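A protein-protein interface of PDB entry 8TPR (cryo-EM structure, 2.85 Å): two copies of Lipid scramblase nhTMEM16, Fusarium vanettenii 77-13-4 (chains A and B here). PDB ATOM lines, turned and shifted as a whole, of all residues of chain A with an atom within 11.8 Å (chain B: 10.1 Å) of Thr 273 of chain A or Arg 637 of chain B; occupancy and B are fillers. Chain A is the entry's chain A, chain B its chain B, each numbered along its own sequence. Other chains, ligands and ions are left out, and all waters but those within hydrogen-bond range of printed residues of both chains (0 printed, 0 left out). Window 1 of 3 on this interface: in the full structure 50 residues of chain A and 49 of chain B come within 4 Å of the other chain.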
ATOM      1  N   LEU A  90      39.823 -10.538 -16.961  1.00  0.00           N
ATOM      2  CA  LEU A  90      38.408 -10.194 -17.047  1.00  0.00           C
ATOM      3  C   LEU A  90      38.065  -9.625 -18.420  1.00  0.00           C
ATOM      4  O   LEU A  90      37.061 -10.016 -19.027  1.00  0.00           O
ATOM      5  CB  LEU A  90      38.047  -9.208 -15.931  1.00  0.00           C
ATOM      6  CG  LEU A  90      36.609  -8.753 -15.650  1.00  0.00           C
ATOM      7  CD1 LEU A  90      36.535  -7.749 -14.503  1.00  0.00           C
ATOM      8  CD2 LEU A  90      35.976  -8.167 -16.900  1.00  0.00           C
ATOM      9  N   HIS A  91      38.894  -8.718 -18.941  1.00  0.00           N
ATOM     10  CA  HIS A  91      38.619  -8.165 -20.265  1.00  0.00           C
ATOM     11  C   HIS A  91      38.940  -9.136 -21.395  1.00  0.00           C
ATOM     12  O   HIS A  91      38.598  -8.846 -22.547  1.00  0.00           O
ATOM     13  CB  HIS A  91      39.373  -6.849 -20.488  1.00  0.00           C
ATOM     14  CG  HIS A  91      39.404  -5.945 -19.294  1.00  0.00           C
ATOM     15  ND1 HIS A  91      40.207  -6.173 -18.200  1.00  0.00           N
ATOM     16  CD2 HIS A  91      38.720  -4.807 -19.026  1.00  0.00           C
ATOM     17  CE1 HIS A  91      40.024  -5.212 -17.312  1.00  0.00           C
ATOM     18  NE2 HIS A  91      39.123  -4.373 -17.788  1.00  0.00           N
ATOM     19  N   GLY A  92      39.581 -10.263 -21.105  1.00  0.00           N
ATOM     20  CA  GLY A  92      39.769 -11.310 -22.087  1.00  0.00           C
ATOM     21  C   GLY A  92      41.097 -11.332 -22.808  1.00  0.00           C
ATOM     22  O   GLY A  92      41.252 -12.116 -23.751  1.00  0.00           O
ATOM     23  N   SER A 254      40.080  -3.673 -27.226  1.00  0.00           N
ATOM     24  CA  SER A 254      38.744  -3.658 -26.641  1.00  0.00           C
ATOM     25  C   SER A 254      38.715  -2.899 -25.321  1.00  0.00           C
ATOM     26  O   SER A 254      37.666  -2.370 -24.934  1.00  0.00           O
ATOM     27  CB  SER A 254      38.242  -5.086 -26.443  1.00  0.00           C
ATOM     28  OG  SER A 254      38.671  -5.926 -27.500  1.00  0.00           O
ATOM     29  N   ILE A 255      39.844  -2.832 -24.617  1.00  0.00           N
ATOM     30  CA  ILE A 255      39.919  -2.153 -23.325  1.00  0.00           C
ATOM     31  C   ILE A 255      39.961  -0.651 -23.599  1.00  0.00           C
ATOM     32  O   ILE A 255      40.995  -0.109 -23.990  1.00  0.00           O
ATOM     33  CB  ILE A 255      41.131  -2.609 -22.509  1.00  0.00           C
ATOM     34  CG1 ILE A 255      41.148  -4.133 -22.385  1.00  0.00           C
ATOM     35  CG2 ILE A 255      41.119  -1.960 -21.135  1.00  0.00           C
ATOM     36  CD1 ILE A 255      42.297  -4.661 -21.560  1.00  0.00           C
ATOM     37  N   GLN A 256      38.836   0.024 -23.389  1.00  0.00           N
ATOM     38  CA  GLN A 256      38.772   1.466 -23.575  1.00  0.00           C
ATOM     39  C   GLN A 256      39.385   2.173 -22.374  1.00  0.00           C
ATOM     40  O   GLN A 256      39.090   1.833 -21.225  1.00  0.00           O
ATOM     41  CB  GLN A 256      37.326   1.917 -23.773  1.00  0.00           C
ATOM     42  CG  GLN A 256      36.851   1.863 -25.213  1.00  0.00           C
ATOM     43  CD  GLN A 256      35.871   0.734 -25.459  1.00  0.00           C
ATOM     44  OE1 GLN A 256      35.054   0.410 -24.598  1.00  0.00           O
ATOM     45  NE2 GLN A 256      35.946   0.132 -26.640  1.00  0.00           N
ATOM     46  N   GLU A 267      27.245  14.019 -15.668  1.00  0.00           N
ATOM     47  CA  GLU A 267      27.413  12.583 -15.496  1.00  0.00           C
ATOM     48  C   GLU A 267      26.043  11.925 -15.529  1.00  0.00           C
ATOM     49  O   GLU A 267      25.144  12.316 -14.775  1.00  0.00           O
ATOM     50  CB  GLU A 267      28.132  12.266 -14.184  1.00  0.00           C
ATOM     51  CG  GLU A 267      29.589  11.875 -14.355  1.00  0.00           C
ATOM     52  CD  GLU A 267      30.302  11.692 -13.032  1.00  0.00           C
ATOM     53  OE1 GLU A 267      29.773  12.161 -12.002  1.00  0.00           O
ATOM     54  OE2 GLU A 267      31.391  11.081 -13.021  1.00  0.00           O
ATOM     55  N   ALA A 268      25.890  10.934 -16.393  1.00  0.00           N
ATOM     56  CA  ALA A 268      24.651  10.189 -16.533  1.00  0.00           C
ATOM     57  C   ALA A 268      24.863   8.754 -16.065  1.00  0.00           C
ATOM     58  O   ALA A 268      25.936   8.380 -15.582  1.00  0.00           O
ATOM     59  CB  ALA A 268      24.156  10.231 -17.979  1.00  0.00           C
ATOM     60  N   GLU A 269      23.818   7.944 -16.210  1.00  0.00           N
ATOM     61  CA  GLU A 269      23.860   6.531 -15.853  1.00  0.00           C
ATOM     62  C   GLU A 269      23.158   5.748 -16.953  1.00  0.00           C
ATOM     63  O   GLU A 269      21.924   5.715 -17.002  1.00  0.00           O
ATOM     64  CB  GLU A 269      23.200   6.283 -14.496  1.00  0.00           C
ATOM     65  N   ASP A 270      23.939   5.131 -17.834  1.00  0.00           N
ATOM     66  CA  ASP A 270      23.365   4.322 -18.895  1.00  0.00           C
ATOM     67  C   ASP A 270      22.600   3.145 -18.295  1.00  0.00           C
ATOM     68  O   ASP A 270      23.098   2.465 -17.392  1.00  0.00           O
ATOM     69  CB  ASP A 270      24.454   3.811 -19.831  1.00  0.00           C
ATOM     70  CG  ASP A 270      25.677   3.313 -19.085  1.00  0.00           C
ATOM     71  OD1 ASP A 270      25.738   3.498 -17.851  1.00  0.00           O
ATOM     72  OD2 ASP A 270      26.577   2.737 -19.732  1.00  0.00           O
ATOM     73  N   PRO A 271      21.390   2.877 -18.779  1.00  0.00           N
ATOM     74  CA  PRO A 271      20.576   1.823 -18.156  1.00  0.00           C
ATOM     75  C   PRO A 271      21.005   0.426 -18.569  1.00  0.00           C
ATOM     76  O   PRO A 271      20.160  -0.433 -18.841  1.00  0.00           O
ATOM     77  CB  PRO A 271      19.154   2.136 -18.646  1.00  0.00           C
ATOM     78  CG  PRO A 271      19.241   3.468 -19.362  1.00  0.00           C
ATOM     79  CD  PRO A 271      20.651   3.599 -19.823  1.00  0.00           C
ATOM     80  N   ILE A 272      22.314   0.182 -18.600  1.00  0.00           N
ATOM     81  CA  ILE A 272      22.853  -1.150 -18.848  1.00  0.00           C
ATOM     82  C   ILE A 272      23.789  -1.507 -17.701  1.00  0.00           C
ATOM     83  O   ILE A 272      23.937  -2.679 -17.341  1.00  0.00           O
ATOM     84  CB  ILE A 272      23.585  -1.213 -20.203  1.00  0.00           C
ATOM     85  CG1 ILE A 272      22.654  -0.802 -21.346  1.00  0.00           C
ATOM     86  CG2 ILE A 272      24.134  -2.609 -20.459  1.00  0.00           C
ATOM     87  CD1 ILE A 272      21.408  -1.649 -21.454  1.00  0.00           C
ATOM     88  N   THR A 273      24.408  -0.488 -17.103  1.00  0.00           N
ATOM     89  CA  THR A 273      25.336  -0.680 -15.993  1.00  0.00           C
ATOM     90  C   THR A 273      25.107   0.382 -14.926  1.00  0.00           C
ATOM     91  O   THR A 273      24.486   1.415 -15.193  1.00  0.00           O
ATOM     92  CB  THR A 273      26.799  -0.624 -16.456  1.00  0.00           C
ATOM     93  OG1 THR A 273      27.224   0.742 -16.541  1.00  0.00           O
ATOM     94  CG2 THR A 273      26.996  -1.300 -17.810  1.00  0.00           C
ATOM     95  N   GLY A 274      25.602   0.139 -13.718  1.00  0.00           N
ATOM     96  CA  GLY A 274      25.534   1.132 -12.669  1.00  0.00           C
ATOM     97  C   GLY A 274      26.621   2.179 -12.703  1.00  0.00           C
ATOM     98  O   GLY A 274      26.641   3.067 -11.845  1.00  0.00           O
ATOM     99  N   GLU A 275      27.529   2.100 -13.669  1.00  0.00           N
ATOM    100  CA  GLU A 275      28.636   3.042 -13.735  1.00  0.00           C
ATOM    101  C   GLU A 275      28.127   4.432 -14.114  1.00  0.00           C
ATOM    102  O   GLU A 275      27.351   4.563 -15.070  1.00  0.00           O
ATOM    103  CB  GLU A 275      29.678   2.570 -14.747  1.00  0.00           C
ATOM    104  N   PRO A 276      28.535   5.482 -13.401  1.00  0.00           N
ATOM    105  CA  PRO A 276      28.116   6.841 -13.769  1.00  0.00           C
ATOM    106  C   PRO A 276      28.914   7.398 -14.938  1.00  0.00           C
ATOM    107  O   PRO A 276      29.928   8.072 -14.737  1.00  0.00           O
ATOM    108  CB  PRO A 276      28.361   7.640 -12.484  1.00  0.00           C
ATOM    109  CG  PRO A 276      29.468   6.912 -11.802  1.00  0.00           C
ATOM    110  CD  PRO A 276      29.321   5.457 -12.157  1.00  0.00           C
ATOM    111  N   VAL A 277      28.475   7.107 -16.163  1.00  0.00           N
ATOM    112  CA  VAL A 277      29.177   7.529 -17.373  1.00  0.00           C
ATOM    113  C   VAL A 277      29.301   9.048 -17.417  1.00  0.00           C
ATOM    114  O   VAL A 277      28.507   9.770 -16.805  1.00  0.00           O
ATOM    115  CB  VAL A 277      28.474   6.992 -18.632  1.00  0.00           C
ATOM    116  CG1 VAL A 277      27.363   7.932 -19.077  1.00  0.00           C
ATOM    117  CG2 VAL A 277      29.481   6.775 -19.752  1.00  0.00           C
ATOM    118  N   LYS A 278      30.302   9.537 -18.146  1.00  0.00           N
ATOM    119  CA  LYS A 278      30.647  10.958 -18.222  1.00  0.00           C
ATOM    120  C   LYS A 278      30.204  11.463 -19.591  1.00  0.00           C
ATOM    121  O   LYS A 278      30.926  11.297 -20.578  1.00  0.00           O
ATOM    122  CB  LYS A 278      32.146  11.143 -18.015  1.00  0.00           C
ATOM    123  CG  LYS A 278      32.570  11.352 -16.570  1.00  0.00           C
ATOM    124  CD  LYS A 278      34.086  11.267 -16.418  1.00  0.00           C
ATOM    125  CE  LYS A 278      34.751  12.631 -16.402  1.00  0.00           C
ATOM    126  NZ  LYS A 278      34.289  13.512 -17.503  1.00  0.00           N
ATOM    127  N   VAL B  95      27.127 -18.212 -21.963  1.00  0.00           N
ATOM    128  CA  VAL B  95      27.643 -17.147 -21.107  1.00  0.00           C
ATOM    129  C   VAL B  95      28.412 -17.732 -19.929  1.00  0.00           C
ATOM    130  O   VAL B  95      29.606 -17.462 -19.747  1.00  0.00           O
ATOM    131  CB  VAL B  95      26.497 -16.237 -20.632  1.00  0.00           C
ATOM    132  CG1 VAL B  95      27.015 -15.204 -19.645  1.00  0.00           C
ATOM    133  CG2 VAL B  95      25.830 -15.562 -21.819  1.00  0.00           C
ATOM    134  N   VAL B 245      22.564 -13.863 -30.673  1.00  0.00           N
ATOM    135  CA  VAL B 245      22.764 -13.522 -29.268  1.00  0.00           C
ATOM    136  C   VAL B 245      21.486 -13.756 -28.473  1.00  0.00           C
ATOM    137  O   VAL B 245      21.526 -14.251 -27.341  1.00  0.00           O
ATOM    138  CB  VAL B 245      23.258 -12.072 -29.134  1.00  0.00           C
ATOM    139  CG1 VAL B 245      23.185 -11.623 -27.688  1.00  0.00           C
ATOM    140  CG2 VAL B 245      24.676 -11.951 -29.662  1.00  0.00           C
ATOM    141  N   LEU B 628      25.602   1.600 -33.600  1.00  0.00           N
ATOM    142  CA  LEU B 628      24.178   1.544 -33.305  1.00  0.00           C
ATOM    143  C   LEU B 628      23.851   0.919 -31.957  1.00  0.00           C
ATOM    144  O   LEU B 628      22.682   0.949 -31.553  1.00  0.00           O
ATOM    145  CB  LEU B 628      23.435   0.773 -34.407  1.00  0.00           C
ATOM    146  CG  LEU B 628      22.947   1.603 -35.596  1.00  0.00           C
ATOM    147  CD1 LEU B 628      21.787   0.907 -36.288  1.00  0.00           C
ATOM    148  CD2 LEU B 628      22.551   3.003 -35.155  1.00  0.00           C
ATOM    149  N   ASP B 629      24.837   0.351 -31.258  1.00  0.00           N
ATOM    150  CA  ASP B 629      24.651  -0.237 -29.929  1.00  0.00           C
ATOM    151  C   ASP B 629      23.584  -1.337 -29.958  1.00  0.00           C
ATOM    152  O   ASP B 629      22.514  -1.234 -29.355  1.00  0.00           O
ATOM    153  CB  ASP B 629      24.298   0.841 -28.898  1.00  0.00           C
ATOM    154  N   SER B 630      23.918  -2.399 -30.682  1.00  0.00           N
ATOM    155  CA  SER B 630      23.013  -3.532 -30.807  1.00  0.00           C
ATOM    156  C   SER B 630      22.837  -4.212 -29.441  1.00  0.00           C
ATOM    157  O   SER B 630      23.751  -4.196 -28.620  1.00  0.00           O
ATOM    158  CB  SER B 630      23.570  -4.531 -31.818  1.00  0.00           C
ATOM    159  OG  SER B 630      23.642  -3.971 -33.118  1.00  0.00           O
ATOM    160  N   PRO B 631      21.653  -4.766 -29.163  1.00  0.00           N
ATOM    161  CA  PRO B 631      21.463  -5.480 -27.896  1.00  0.00           C
ATOM    162  C   PRO B 631      22.515  -6.527 -27.547  1.00  0.00           C
ATOM    163  O   PRO B 631      22.782  -6.729 -26.354  1.00  0.00           O
ATOM    164  CB  PRO B 631      20.085  -6.118 -28.113  1.00  0.00           C
ATOM    165  CG  PRO B 631      19.373  -5.128 -29.139  1.00  0.00           C
ATOM    166  CD  PRO B 631      20.389  -4.042 -29.370  1.00  0.00           C
ATOM    167  N   GLY B 632      23.105  -7.211 -28.522  1.00  0.00           N
ATOM    168  CA  GLY B 632      24.106  -8.211 -28.191  1.00  0.00           C
ATOM    169  C   GLY B 632      25.285  -7.630 -27.437  1.00  0.00           C
ATOM    170  O   GLY B 632      25.766  -8.217 -26.465  1.00  0.00           O
ATOM    171  N   LEU B 633      25.752  -6.454 -27.862  1.00  0.00           N
ATOM    172  CA  LEU B 633      26.925  -5.849 -27.238  1.00  0.00           C
ATOM    173  C   LEU B 633      26.645  -5.432 -25.801  1.00  0.00           C
ATOM    174  O   LEU B 633      27.456  -5.696 -24.903  1.00  0.00           O
ATOM    175  CB  LEU B 633      27.397  -4.655 -28.066  1.00  0.00           C
ATOM    176  N   GLN B 634      25.511  -4.767 -25.558  1.00  0.00           N
ATOM    177  CA  GLN B 634      25.230  -4.348 -24.190  1.00  0.00           C
ATOM    178  C   GLN B 634      24.924  -5.550 -23.312  1.00  0.00           C
ATOM    179  O   GLN B 634      25.281  -5.564 -22.132  1.00  0.00           O
ATOM    180  CB  GLN B 634      24.094  -3.320 -24.129  1.00  0.00           C
ATOM    181  CG  GLN B 634      22.676  -3.866 -24.106  1.00  0.00           C
ATOM    182  CD  GLN B 634      21.702  -2.978 -24.853  1.00  0.00           C
ATOM    183  OE1 GLN B 634      21.703  -1.762 -24.681  1.00  0.00           O
ATOM    184  NE2 GLN B 634      20.836  -3.582 -25.641  1.00  0.00           N
ATOM    185  N   LYS B 635      24.289  -6.585 -23.873  1.00  0.00           N
ATOM    186  CA  LYS B 635      24.069  -7.805 -23.103  1.00  0.00           C
ATOM    187  C   LYS B 635      25.394  -8.447 -22.706  1.00  0.00           C
ATOM    188  O   LYS B 635      25.566  -8.879 -21.559  1.00  0.00           O
ATOM    189  CB  LYS B 635      23.214  -8.785 -23.905  1.00  0.00           C
ATOM    190  N   GLU B 636      26.350  -8.501 -23.637  1.00  0.00           N
ATOM    191  CA  GLU B 636      27.659  -9.065 -23.335  1.00  0.00           C
ATOM    192  C   GLU B 636      28.417  -8.255 -22.293  1.00  0.00           C
ATOM    193  O   GLU B 636      28.990  -8.837 -21.366  1.00  0.00           O
ATOM    194  CB  GLU B 636      28.491  -9.174 -24.612  1.00  0.00           C
ATOM    195  N   ARG B 637      28.433  -6.927 -22.412  1.00  0.00           N
ATOM    196  CA  ARG B 637      29.137  -6.097 -21.444  1.00  0.00           C
ATOM    197  C   ARG B 637      28.405  -6.008 -20.113  1.00  0.00           C
ATOM    198  O   ARG B 637      29.007  -5.650 -19.097  1.00  0.00           O
ATOM    199  CB  ARG B 637      29.387  -4.688 -22.005  1.00  0.00           C
ATOM    200  CG  ARG B 637      28.149  -3.849 -22.241  1.00  0.00           C
ATOM    201  CD  ARG B 637      28.507  -2.574 -22.990  1.00  0.00           C
ATOM    202  NE  ARG B 637      27.339  -1.746 -23.275  1.00  0.00           N
ATOM    203  CZ  ARG B 637      26.851  -0.832 -22.452  1.00  0.00           C
ATOM    204  NH1 ARG B 637      27.394  -0.605 -21.267  1.00  0.00           N
ATOM    205  NH2 ARG B 637      25.788  -0.124 -22.826  1.00  0.00           N
ATOM    206  N   LYS B 638      27.110  -6.328 -20.094  1.00  0.00           N
ATOM    207  CA  LYS B 638      26.362  -6.461 -18.853  1.00  0.00           C
ATOM    208  C   LYS B 638      26.741  -7.759 -18.162  1.00  0.00           C
ATOM    209  O   LYS B 638      26.934  -7.788 -16.944  1.00  0.00           O
ATOM    210  CB  LYS B 638      24.857  -6.426 -19.128  1.00  0.00           C
ATOM    211  CG  LYS B 638      24.046  -5.693 -18.077  1.00  0.00           C
ATOM    212  CD  LYS B 638      22.683  -6.340 -17.884  1.00  0.00           C
ATOM    213  CE  LYS B 638      21.782  -6.102 -19.085  1.00  0.00           C
ATOM    214  NZ  LYS B 638      20.393  -5.749 -18.678  1.00  0.00           N
ATOM    215  N   GLU B 639      26.846  -8.842 -18.937  1.00  0.00           N
ATOM    216  CA  GLU B 639      27.286 -10.112 -18.372  1.00  0.00           C
ATOM    217  C   GLU B 639      28.700 -10.002 -17.818  1.00  0.00           C
ATOM    218  O   GLU B 639      28.995 -10.515 -16.734  1.00  0.00           O
ATOM    219  CB  GLU B 639      27.204 -11.214 -19.428  1.00  0.00           C
ATOM    220  N   ARG B 640      29.588  -9.326 -18.552  1.00  0.00           N
ATOM    221  CA  ARG B 640      30.948  -9.122 -18.065  1.00  0.00           C
ATOM    222  C   ARG B 640      30.960  -8.299 -16.783  1.00  0.00           C
ATOM    223  O   ARG B 640      31.702  -8.609 -15.842  1.00  0.00           O
ATOM    224  CB  ARG B 640      31.797  -8.450 -19.144  1.00  0.00           C
ATOM    225  N   PHE B 641      30.145  -7.244 -16.727  1.00  0.00           N
ATOM    226  CA  PHE B 641      30.086  -6.414 -15.526  1.00  0.00           C
ATOM    227  C   PHE B 641      29.555  -7.198 -14.333  1.00  0.00           C
ATOM    228  O   PHE B 641      30.065  -7.060 -13.215  1.00  0.00           O
ATOM    229  CB  PHE B 641      29.221  -5.180 -15.786  1.00  0.00           C
ATOM    230  CG  PHE B 641      29.555  -4.011 -14.906  1.00  0.00           C
ATOM    231  CD1 PHE B 641      30.727  -3.299 -15.093  1.00  0.00           C
ATOM    232  CD2 PHE B 641      28.695  -3.619 -13.896  1.00  0.00           C
ATOM    233  CE1 PHE B 641      31.036  -2.221 -14.286  1.00  0.00           C
ATOM    234  CE2 PHE B 641      28.998  -2.543 -13.085  1.00  0.00           C
ATOM    235  CZ  PHE B 641      30.169  -1.843 -13.280  1.00  0.00           C
ATOM    236  N   GLN B 642      28.525  -8.023 -14.549  1.00  0.00           N
ATOM    237  CA  GLN B 642      28.003  -8.855 -13.470  1.00  0.00           C
ATOM    238  C   GLN B 642      29.030  -9.881 -13.009  1.00  0.00           C
ATOM    239  O   GLN B 642      29.124 -10.163 -11.810  1.00  0.00           O
ATOM    240  CB  GLN B 642      26.717  -9.553 -13.910  1.00  0.00           C
ATOM    241  CG  GLN B 642      25.583  -8.609 -14.273  1.00  0.00           C
ATOM    242  CD  GLN B 642      25.036  -7.854 -13.080  1.00  0.00           C
ATOM    243  OE1 GLN B 642      25.206  -8.270 -11.932  1.00  0.00           O
ATOM    244  NE2 GLN B 642      24.372  -6.735 -13.342  1.00  0.00           N
ATOM    245  N   THR B 643      29.796 -10.452 -13.940  1.00  0.00           N
ATOM    246  CA  THR B 643      30.876 -11.355 -13.566  1.00  0.00           C
ATOM    247  C   THR B 643      31.958 -10.647 -12.759  1.00  0.00           C
ATOM    248  O   THR B 643      32.491 -11.234 -11.811  1.00  0.00           O
ATOM    249  CB  THR B 643      31.476 -11.997 -14.819  1.00  0.00           C
ATOM    250  OG1 THR B 643      30.538 -12.929 -15.374  1.00  0.00           O
ATOM    251  CG2 THR B 643      32.768 -12.735 -14.494  1.00  0.00           C
ATOM    252  N   LYS B 644      32.275  -9.404 -13.104  1.00  0.00           N
ATOM    253  CA  LYS B 644      33.240  -8.612 -12.347  1.00  0.00           C
ATOM    254  C   LYS B 644      32.799  -8.425 -10.899  1.00  0.00           C
ATOM    255  O   LYS B 644      31.604  -8.361 -10.609  1.00  0.00           O
ATOM    256  CB  LYS B 644      33.446  -7.249 -13.006  1.00  0.00           C
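Of the printed residues of chain B, Leu 90 of chain A touches Lys 644. Asp 270 of chain A touches just one residue of chain B: Arg 637. Of chain B, only Gln 634 (3.2 Å), Arg 637 (3.5 Å) and Lys 638 (3.1 Å) come within 4 Å of Ile 272 of chain A. Of chain B, only Arg 637 (3.5 Å) comes within 4 Å of Thr 273 of chain A. No residue of chain B comes within 4 Å of Gly 274 of chain A. Asp 629 of chain B touches none of the printed residues of chain A. No residue of chain A comes within 4 Å of Leu 633 of chain B. Of chain A, only Ile 272 (3.2 Å) comes within 4 Å of Gln 634 of chain B. No residue of chain A comes within 4 Å of Lys 635 of chain B. No residue of chain A comes within 4 Å of Glu 636 of chain B. Of chain A, only Asp 270, Ile 272 and Thr 273 come within 4 Å of Arg 637 of chain B. Of chain A, only Ile 272 comes within 4 Å of Lys 638 of chain B. No residue of chain A comes within 4 Å of Glu 639 of chain B. No residue of chain A comes within 4 Å of Phe 641 of chain B. Of the printed residues of chain A, Lys 644 of chain B touches Leu 90. The nearest residue of chain A that does not touch Arg 637 of chain B is Pro 271 of chain A (6.4 Å). The nearest printed residue of chain A that does not touch Lys 644 of chain B is His 91 of chain A (8.0 Å).
The side-chain carboxylate (OD2) of Asp 270 of chain A is in salt-bridge range of the guanidinium group (NH1) of Arg 637 of chain B, at 3.8 Å.
Of the 18 printed residues of chain A, 4 touch a printed residue of chain B. Hydrophobic or aromatic side chains of chain A that line the printed part of chain B: Leu 90 and Ile 272. Among the printed residues, 6 pairs touch across the chains. Among the printed residues, Asp or Glu carboxylates within 4 Å of a Lys or Arg side-chain nitrogen of the other chain: Asp 270 of chain A with Arg 637 of chain B (3.8 Å).
The side-chain carboxylate (OD1) of Asp 270 of chain A lies within hydrogen-bond range of the side-chain hydroxyl (OG1) of Thr 273 of chain A (3.4 Å). The side-chain hydroxyl (OG1) of Thr 273 of chain A is in hydrogen-bond range of the backbone NH (N) of Glu 275 of chain A.
Among the printed residues, merely in contact across the chains: Leu 90 of chain A with Lys 644 of chain B, Ile 272 of chain A with Gln 634 of chain B, Ile 272 of chain A with Arg 637 of chain B, Ile 272 of chain A with Lys 638 of chain B and Thr 273 of chain A with Arg 637 of chain B.
No position is printed for both chains.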
